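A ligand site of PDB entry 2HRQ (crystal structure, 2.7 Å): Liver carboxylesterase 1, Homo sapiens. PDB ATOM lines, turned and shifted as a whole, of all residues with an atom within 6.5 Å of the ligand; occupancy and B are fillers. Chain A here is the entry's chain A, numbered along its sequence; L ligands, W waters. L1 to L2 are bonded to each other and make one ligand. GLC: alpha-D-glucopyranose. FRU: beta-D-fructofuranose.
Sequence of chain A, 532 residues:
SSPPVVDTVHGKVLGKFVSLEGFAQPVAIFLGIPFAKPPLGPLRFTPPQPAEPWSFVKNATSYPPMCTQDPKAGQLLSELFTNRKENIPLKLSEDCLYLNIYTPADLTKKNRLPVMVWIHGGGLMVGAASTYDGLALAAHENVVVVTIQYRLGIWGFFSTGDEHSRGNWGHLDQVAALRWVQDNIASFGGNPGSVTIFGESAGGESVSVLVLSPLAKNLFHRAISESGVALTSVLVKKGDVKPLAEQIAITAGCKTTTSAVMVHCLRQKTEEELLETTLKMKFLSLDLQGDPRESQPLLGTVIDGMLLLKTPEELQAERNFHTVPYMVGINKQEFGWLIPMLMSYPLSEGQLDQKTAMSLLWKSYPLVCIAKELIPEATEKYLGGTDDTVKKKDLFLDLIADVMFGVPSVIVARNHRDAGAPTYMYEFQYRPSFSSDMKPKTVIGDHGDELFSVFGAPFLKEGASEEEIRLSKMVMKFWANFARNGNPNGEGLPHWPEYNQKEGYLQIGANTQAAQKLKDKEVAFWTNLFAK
NE1 of Trp 337 is in hydrogen-bond range of O of Met 438 (3.0 Å). OD1 of Asp 394 is in salt-bridge range of NZ of Lys 393 (2.9 Å).
Trp 337 touches the ligand. CA of Met 341 touches O6 of GLC L1, at 3.8 Å. Gly 350 touches the ligand. Leu 397 touches the ligand. Met 438 touches the ligand. Hydrophobic or aromatic side chains that line the ligand: Trp 337 and Leu 397.
The backbone carbonyl oxygen (O) of Ser 348 lies close to an oxygen (O1) of FRU L2 (3.3 Å). The side-chain amino group (NZ) of Lys 393 lies within hydrogen-bond range of an oxygen (O3) of GLC L1 (2.9 Å). An oxygen (O4) of GLC L1 sits at hydrogen-bond distance from the backbone carbonyl oxygen of Gly 336, at 2.7 Å. O of Leu 347 sits close to O1 of FRU L2 (3.5 Å).
Water W2 lies within hydrogen-bond range of the indole nitrogen of Trp 337 and an oxygen (O6) of GLC L1. Water W1 lies within hydrogen-bond range of the side-chain hydroxyl (OG) of Ser 348 and an oxygen (O1) of FRU L2.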
ATOM      1  N   PHE A 335      11.496  -0.538  11.491  1.00  0.00           N
ATOM      2  CA  PHE A 335      10.457  -0.247  10.510  1.00  0.00           C
ATOM      3  C   PHE A 335       9.657  -1.508  10.176  1.00  0.00           C
ATOM      4  O   PHE A 335       9.048  -1.613   9.111  1.00  0.00           O
ATOM      5  CB  PHE A 335      11.089   0.313   9.242  1.00  0.00           C
ATOM      6  CG  PHE A 335      10.265   1.374   8.566  1.00  0.00           C
ATOM      7  CD1 PHE A 335       9.831   1.219   7.260  1.00  0.00           C
ATOM      8  CD2 PHE A 335       9.929   2.540   9.250  1.00  0.00           C
ATOM      9  CE1 PHE A 335       9.075   2.212   6.633  1.00  0.00           C
ATOM     10  CE2 PHE A 335       9.183   3.536   8.633  1.00  0.00           C
ATOM     11  CZ  PHE A 335       8.751   3.371   7.319  1.00  0.00           C
ATOM     12  N   GLY A 336       9.667  -2.459  11.108  1.00  0.00           N
ATOM     13  CA  GLY A 336       8.967  -3.711  10.907  1.00  0.00           C
ATOM     14  C   GLY A 336       7.485  -3.625  10.609  1.00  0.00           C
ATOM     15  O   GLY A 336       7.020  -4.188   9.615  1.00  0.00           O
ATOM     16  N   TRP A 337       6.729  -2.923  11.452  1.00  0.00           N
ATOM     17  CA  TRP A 337       5.289  -2.831  11.253  1.00  0.00           C
ATOM     18  C   TRP A 337       4.611  -1.539  11.728  1.00  0.00           C
ATOM     19  O   TRP A 337       3.912  -0.878  10.959  1.00  0.00           O
ATOM     20  CB  TRP A 337       4.598  -4.008  11.944  1.00  0.00           C
ATOM     21  CG  TRP A 337       3.111  -3.899  11.956  1.00  0.00           C
ATOM     22  CD1 TRP A 337       2.253  -4.213  10.928  1.00  0.00           C
ATOM     23  CD2 TRP A 337       2.283  -3.398  13.016  1.00  0.00           C
ATOM     24  NE1 TRP A 337       0.957  -3.937  11.294  1.00  0.00           N
ATOM     25  CE2 TRP A 337       0.941  -3.438  12.568  1.00  0.00           C
ATOM     26  CE3 TRP A 337       2.547  -2.919  14.312  1.00  0.00           C
ATOM     27  CZ2 TRP A 337      -0.130  -3.023  13.356  1.00  0.00           C
ATOM     28  CZ3 TRP A 337       1.482  -2.496  15.102  1.00  0.00           C
ATOM     29  CH2 TRP A 337       0.159  -2.551  14.620  1.00  0.00           C
ATOM     30  N   LEU A 338       4.814  -1.211  13.002  1.00  0.00           N
ATOM     31  CA  LEU A 338       4.179  -0.041  13.599  1.00  0.00           C
ATOM     32  C   LEU A 338       4.316   1.276  12.845  1.00  0.00           C
ATOM     33  O   LEU A 338       3.307   1.945  12.580  1.00  0.00           O
ATOM     34  CB  LEU A 338       4.656   0.129  15.049  1.00  0.00           C
ATOM     35  CG  LEU A 338       3.905   1.179  15.888  1.00  0.00           C
ATOM     36  CD1 LEU A 338       3.566   0.606  17.255  1.00  0.00           C
ATOM     37  CD2 LEU A 338       4.753   2.428  16.040  1.00  0.00           C
ATOM     38  N   PRO A 340       5.278   1.910   9.574  1.00  0.00           N
ATOM     39  CA  PRO A 340       4.635   1.875   8.255  1.00  0.00           C
ATOM     40  C   PRO A 340       3.109   1.892   8.377  1.00  0.00           C
ATOM     41  O   PRO A 340       2.427   2.631   7.675  1.00  0.00           O
ATOM     42  CB  PRO A 340       5.161   0.583   7.644  1.00  0.00           C
ATOM     43  CG  PRO A 340       6.521   0.470   8.248  1.00  0.00           C
ATOM     44  CD  PRO A 340       6.265   0.813   9.694  1.00  0.00           C
ATOM     45  N   MET A 341       2.588   1.069   9.277  1.00  0.00           N
ATOM     46  CA  MET A 341       1.148   0.978   9.504  1.00  0.00           C
ATOM     47  C   MET A 341       0.550   2.330   9.852  1.00  0.00           C
ATOM     48  O   MET A 341      -0.519   2.691   9.358  1.00  0.00           O
ATOM     49  CB  MET A 341       0.854  -0.032  10.615  1.00  0.00           C
ATOM     50  CG  MET A 341      -0.617  -0.140  11.008  1.00  0.00           C
ATOM     51  SD  MET A 341      -1.194   1.216  12.049  1.00  0.00           S
ATOM     52  CE  MET A 341      -0.561   0.696  13.638  1.00  0.00           C
ATOM     53  N   LEU A 342       1.232   3.075  10.717  1.00  0.00           N
ATOM     54  CA  LEU A 342       0.761   4.388  11.139  1.00  0.00           C
ATOM     55  C   LEU A 342       0.843   5.421  10.020  1.00  0.00           C
ATOM     56  O   LEU A 342      -0.120   6.134   9.758  1.00  0.00           O
ATOM     57  CB  LEU A 342       1.557   4.878  12.356  1.00  0.00           C
ATOM     58  CG  LEU A 342       1.287   4.185  13.697  1.00  0.00           C
ATOM     59  CD1 LEU A 342       2.033   4.917  14.809  1.00  0.00           C
ATOM     60  CD2 LEU A 342      -0.210   4.173  13.982  1.00  0.00           C
ATOM     61  N   TYR A 345       1.700   3.149   4.747  1.00  0.00           N
ATOM     62  CA  TYR A 345       2.635   2.864   3.671  1.00  0.00           C
ATOM     63  C   TYR A 345       1.965   1.964   2.645  1.00  0.00           C
ATOM     64  O   TYR A 345       1.204   1.061   2.997  1.00  0.00           O
ATOM     65  CB  TYR A 345       3.888   2.194   4.216  1.00  0.00           C
ATOM     66  CG  TYR A 345       5.093   3.075   4.134  1.00  0.00           C
ATOM     67  CD1 TYR A 345       5.135   4.276   4.819  1.00  0.00           C
ATOM     68  CD2 TYR A 345       6.185   2.720   3.345  1.00  0.00           C
ATOM     69  CE1 TYR A 345       6.232   5.118   4.722  1.00  0.00           C
ATOM     70  CE2 TYR A 345       7.279   3.543   3.237  1.00  0.00           C
ATOM     71  CZ  TYR A 345       7.304   4.743   3.918  1.00  0.00           C
ATOM     72  OH  TYR A 345       8.384   5.584   3.817  1.00  0.00           O
ATOM     73  N   LEU A 347       2.267  -0.750   1.165  1.00  0.00           N
ATOM     74  CA  LEU A 347       2.852  -2.090   1.138  1.00  0.00           C
ATOM     75  C   LEU A 347       1.732  -3.115   1.290  1.00  0.00           C
ATOM     76  O   LEU A 347       1.955  -4.247   1.728  1.00  0.00           O
ATOM     77  CB  LEU A 347       3.864  -2.251   2.272  1.00  0.00           C
ATOM     78  CG  LEU A 347       5.074  -1.318   2.287  1.00  0.00           C
ATOM     79  CD1 LEU A 347       5.930  -1.613   3.506  1.00  0.00           C
ATOM     80  CD2 LEU A 347       5.893  -1.502   1.025  1.00  0.00           C
ATOM     81  N   SER A 348       0.527  -2.723   0.895  1.00  0.00           N
ATOM     82  CA  SER A 348      -0.649  -3.580   1.002  1.00  0.00           C
ATOM     83  C   SER A 348      -0.557  -4.950   0.328  1.00  0.00           C
ATOM     84  O   SER A 348      -1.338  -5.854   0.639  1.00  0.00           O
ATOM     85  CB  SER A 348      -1.869  -2.828   0.477  1.00  0.00           C
ATOM     86  OG  SER A 348      -3.043  -3.594   0.643  1.00  0.00           O
ATOM     87  N   GLU A 349       0.382  -5.124  -0.598  1.00  0.00           N
ATOM     88  CA  GLU A 349       0.512  -6.401  -1.302  1.00  0.00           C
ATOM     89  C   GLU A 349       1.496  -7.379  -0.665  1.00  0.00           C
ATOM     90  O   GLU A 349       1.403  -8.586  -0.887  1.00  0.00           O
ATOM     91  CB  GLU A 349       0.909  -6.162  -2.759  1.00  0.00           C
ATOM     92  CG  GLU A 349      -0.128  -5.416  -3.567  1.00  0.00           C
ATOM     93  CD  GLU A 349       0.242  -5.326  -5.039  1.00  0.00           C
ATOM     94  OE1 GLU A 349       1.347  -4.825  -5.348  1.00  0.00           O
ATOM     95  OE2 GLU A 349      -0.571  -5.757  -5.877  1.00  0.00           O
ATOM     96  N   GLY A 350       2.439  -6.851   0.107  1.00  0.00           N
ATOM     97  CA  GLY A 350       3.432  -7.711   0.734  1.00  0.00           C
ATOM     98  C   GLY A 350       4.567  -8.007  -0.227  1.00  0.00           C
ATOM     99  O   GLY A 350       5.571  -8.608   0.150  1.00  0.00           O
ATOM    100  N   GLN A 351       4.416  -7.567  -1.473  1.00  0.00           N
ATOM    101  CA  GLN A 351       5.439  -7.768  -2.480  1.00  0.00           C
ATOM    102  C   GLN A 351       5.979  -6.440  -2.999  1.00  0.00           C
ATOM    103  O   GLN A 351       5.261  -5.440  -3.060  1.00  0.00           O
ATOM    104  CB  GLN A 351       4.869  -8.592  -3.648  1.00  0.00           C
ATOM    105  CG  GLN A 351       4.373  -9.965  -3.237  1.00  0.00           C
ATOM    106  CD  GLN A 351       3.948 -10.827  -4.408  1.00  0.00           C
ATOM    107  OE1 GLN A 351       4.733 -11.066  -5.327  1.00  0.00           O
ATOM    108  NE2 GLN A 351       2.711 -11.310  -4.381  1.00  0.00           N
ATOM    109  N   LYS A 393      10.686  -6.785  -0.231  1.00  0.00           N
ATOM    110  CA  LYS A 393       9.887  -5.959   0.650  1.00  0.00           C
ATOM    111  C   LYS A 393      10.494  -5.900   2.045  1.00  0.00           C
ATOM    112  O   LYS A 393      10.531  -4.836   2.671  1.00  0.00           O
ATOM    113  CB  LYS A 393       8.454  -6.515   0.718  1.00  0.00           C
ATOM    114  CG  LYS A 393       7.518  -5.724   1.631  1.00  0.00           C
ATOM    115  CD  LYS A 393       7.528  -6.229   3.063  1.00  0.00           C
ATOM    116  CE  LYS A 393       6.915  -7.619   3.160  1.00  0.00           C
ATOM    117  NZ  LYS A 393       6.791  -8.072   4.571  1.00  0.00           N
ATOM    118  N   ASP A 394      10.984  -7.041   2.533  1.00  0.00           N
ATOM    119  CA  ASP A 394      11.588  -7.093   3.858  1.00  0.00           C
ATOM    120  C   ASP A 394      12.905  -6.342   3.905  1.00  0.00           C
ATOM    121  O   ASP A 394      13.142  -5.556   4.818  1.00  0.00           O
ATOM    122  CB  ASP A 394      11.827  -8.543   4.280  1.00  0.00           C
ATOM    123  CG  ASP A 394      10.542  -9.320   4.463  1.00  0.00           C
ATOM    124  OD1 ASP A 394       9.539  -8.738   4.948  1.00  0.00           O
ATOM    125  OD2 ASP A 394      10.533 -10.522   4.129  1.00  0.00           O
ATOM    126  N   LEU A 397      12.457  -2.778   4.255  1.00  0.00           N
ATOM    127  CA  LEU A 397      12.150  -2.370   5.626  1.00  0.00           C
ATOM    128  C   LEU A 397      13.436  -2.245   6.441  1.00  0.00           C
ATOM    129  O   LEU A 397      13.525  -1.382   7.319  1.00  0.00           O
ATOM    130  CB  LEU A 397      11.211  -3.374   6.283  1.00  0.00           C
ATOM    131  CG  LEU A 397       9.898  -3.647   5.535  1.00  0.00           C
ATOM    132  CD1 LEU A 397       9.014  -4.575   6.354  1.00  0.00           C
ATOM    133  CD2 LEU A 397       9.165  -2.345   5.253  1.00  0.00           C
ATOM    134  N   ASP A 437      -2.860  -7.585  17.126  1.00  0.00           N
ATOM    135  CA  ASP A 437      -3.243  -8.734  16.315  1.00  0.00           C
ATOM    136  C   ASP A 437      -2.996  -8.525  14.820  1.00  0.00           C
ATOM    137  O   ASP A 437      -2.809  -9.487  14.076  1.00  0.00           O
ATOM    138  CB  ASP A 437      -4.724  -9.062  16.532  1.00  0.00           C
ATOM    139  CG  ASP A 437      -5.127  -8.996  17.991  1.00  0.00           C
ATOM    140  OD1 ASP A 437      -4.401  -9.575  18.837  1.00  0.00           O
ATOM    141  OD2 ASP A 437      -6.164  -8.360  18.279  1.00  0.00           O
ATOM    142  N   MET A 438      -3.009  -7.261  14.398  1.00  0.00           N
ATOM    143  CA  MET A 438      -2.802  -6.912  13.003  1.00  0.00           C
ATOM    144  C   MET A 438      -1.323  -6.784  12.645  1.00  0.00           C
ATOM    145  O   MET A 438      -0.964  -6.193  11.637  1.00  0.00           O
ATOM    146  CB  MET A 438      -3.524  -5.598  12.696  1.00  0.00           C
ATOM    147  CG  MET A 438      -5.030  -5.681  12.953  1.00  0.00           C
ATOM    148  SD  MET A 438      -5.867  -4.081  13.031  1.00  0.00           S
ATOM    149  CE  MET A 438      -5.716  -3.687  14.816  1.00  0.00           C
ATOM    150  N   LYS A 439      -0.478  -7.362  13.488  1.00  0.00           N
ATOM    151  CA  LYS A 439       0.966  -7.310  13.301  1.00  0.00           C
ATOM    152  C   LYS A 439       1.531  -8.648  12.809  1.00  0.00           C
ATOM    153  O   LYS A 439       1.436  -9.661  13.510  1.00  0.00           O
ATOM    154  CB  LYS A 439       1.624  -6.910  14.620  1.00  0.00           C
ATOM    155  CG  LYS A 439       3.143  -6.926  14.637  1.00  0.00           C
ATOM    156  CD  LYS A 439       3.637  -6.735  16.063  1.00  0.00           C
ATOM    157  CE  LYS A 439       5.155  -6.649  16.147  1.00  0.00           C
ATOM    158  NZ  LYS A 439       5.620  -6.481  17.549  1.00  0.00           N
ATOM    159  N   PRO A 440       2.128  -8.667  11.611  1.00  0.00           N
ATOM    160  CA  PRO A 440       2.699  -9.920  11.104  1.00  0.00           C
ATOM    161  C   PRO A 440       3.602 -10.598  12.128  1.00  0.00           C
ATOM    162  O   PRO A 440       4.614 -10.038  12.561  1.00  0.00           O
ATOM    163  CB  PRO A 440       3.444  -9.476   9.828  1.00  0.00           C
ATOM    164  CG  PRO A 440       3.579  -7.982   9.971  1.00  0.00           C
ATOM    165  CD  PRO A 440       2.302  -7.585  10.631  1.00  0.00           C
ATOM    166  N   THR A 442       5.835 -12.564  11.992  1.00  0.00           N
ATOM    167  CA  THR A 442       7.234 -12.719  11.617  1.00  0.00           C
ATOM    168  C   THR A 442       8.062 -11.526  12.129  1.00  0.00           C
ATOM    169  O   THR A 442       9.292 -11.578  12.172  1.00  0.00           O
ATOM    170  CB  THR A 442       7.392 -12.802  10.064  1.00  0.00           C
ATOM    171  OG1 THR A 442       7.070 -11.539   9.464  1.00  0.00           O
ATOM    172  CG2 THR A 442       6.464 -13.872   9.505  1.00  0.00           C
ATOM    173  N   VAL A 443       7.377 -10.459  12.517  1.00  0.00           N
ATOM    174  CA  VAL A 443       8.035  -9.255  13.016  1.00  0.00           C
ATOM    175  C   VAL A 443       8.505  -9.371  14.470  1.00  0.00           C
ATOM    176  O   VAL A 443       7.710  -9.556  15.373  1.00  0.00           O
ATOM    177  CB  VAL A 443       7.080  -8.049  12.868  1.00  0.00           C
ATOM    178  CG1 VAL A 443       7.756  -6.781  13.359  1.00  0.00           C
ATOM    179  CG2 VAL A 443       6.662  -7.905  11.415  1.00  0.00           C
HETATM  180  C1  GLC L   1       2.394  -5.226   4.858  1.00  0.00           C
HETATM  181  C2  GLC L   1       3.904  -5.572   4.865  1.00  0.00           C
HETATM  182  C3  GLC L   1       4.393  -5.681   6.340  1.00  0.00           C
HETATM  183  C4  GLC L   1       4.173  -4.351   7.009  1.00  0.00           C
HETATM  184  C5  GLC L   1       2.664  -3.979   6.991  1.00  0.00           C
HETATM  185  C6  GLC L   1       2.418  -2.603   7.640  1.00  0.00           C
HETATM  186  O2  GLC L   1       4.086  -6.813   4.142  1.00  0.00           O
HETATM  187  O3  GLC L   1       5.780  -6.022   6.343  1.00  0.00           O
HETATM  188  O4  GLC L   1       4.634  -4.441   8.393  1.00  0.00           O
HETATM  189  O5  GLC L   1       2.221  -3.943   5.589  1.00  0.00           O
HETATM  190  O6  GLC L   1       1.208  -2.012   7.151  1.00  0.00           O
HETATM  191  C1  FRU L   2      -0.172  -6.390   3.829  1.00  0.00           C
HETATM  192  C2  FRU L   2       0.290  -6.708   5.250  1.00  0.00           C
HETATM  193  C3  FRU L   2       0.200  -8.215   5.642  1.00  0.00           C
HETATM  194  C4  FRU L   2      -0.157  -8.155   7.110  1.00  0.00           C
HETATM  195  C5  FRU L   2      -1.183  -7.017   7.053  1.00  0.00           C
HETATM  196  C6  FRU L   2      -1.615  -6.356   8.356  1.00  0.00           C
HETATM  197  O1  FRU L   2      -0.703  -5.064   3.829  1.00  0.00           O
HETATM  198  O2  FRU L   2       1.697  -6.310   5.533  1.00  0.00           O
HETATM  199  O3  FRU L   2       1.425  -8.901   5.424  1.00  0.00           O
HETATM  200  O4  FRU L   2      -0.714  -9.415   7.511  1.00  0.00           O
HETATM  201  O5  FRU L   2      -0.587  -6.049   6.162  1.00  0.00           O
HETATM  202  O6  FRU L   2      -2.962  -6.597   8.697  1.00  0.00           O
HETATM  203  O   HOH W   1      -2.868  -2.634   3.509  1.00  0.00           O
HETATM  204  O   HOH W   2      -0.830  -3.391   8.965  1.00  0.00           O
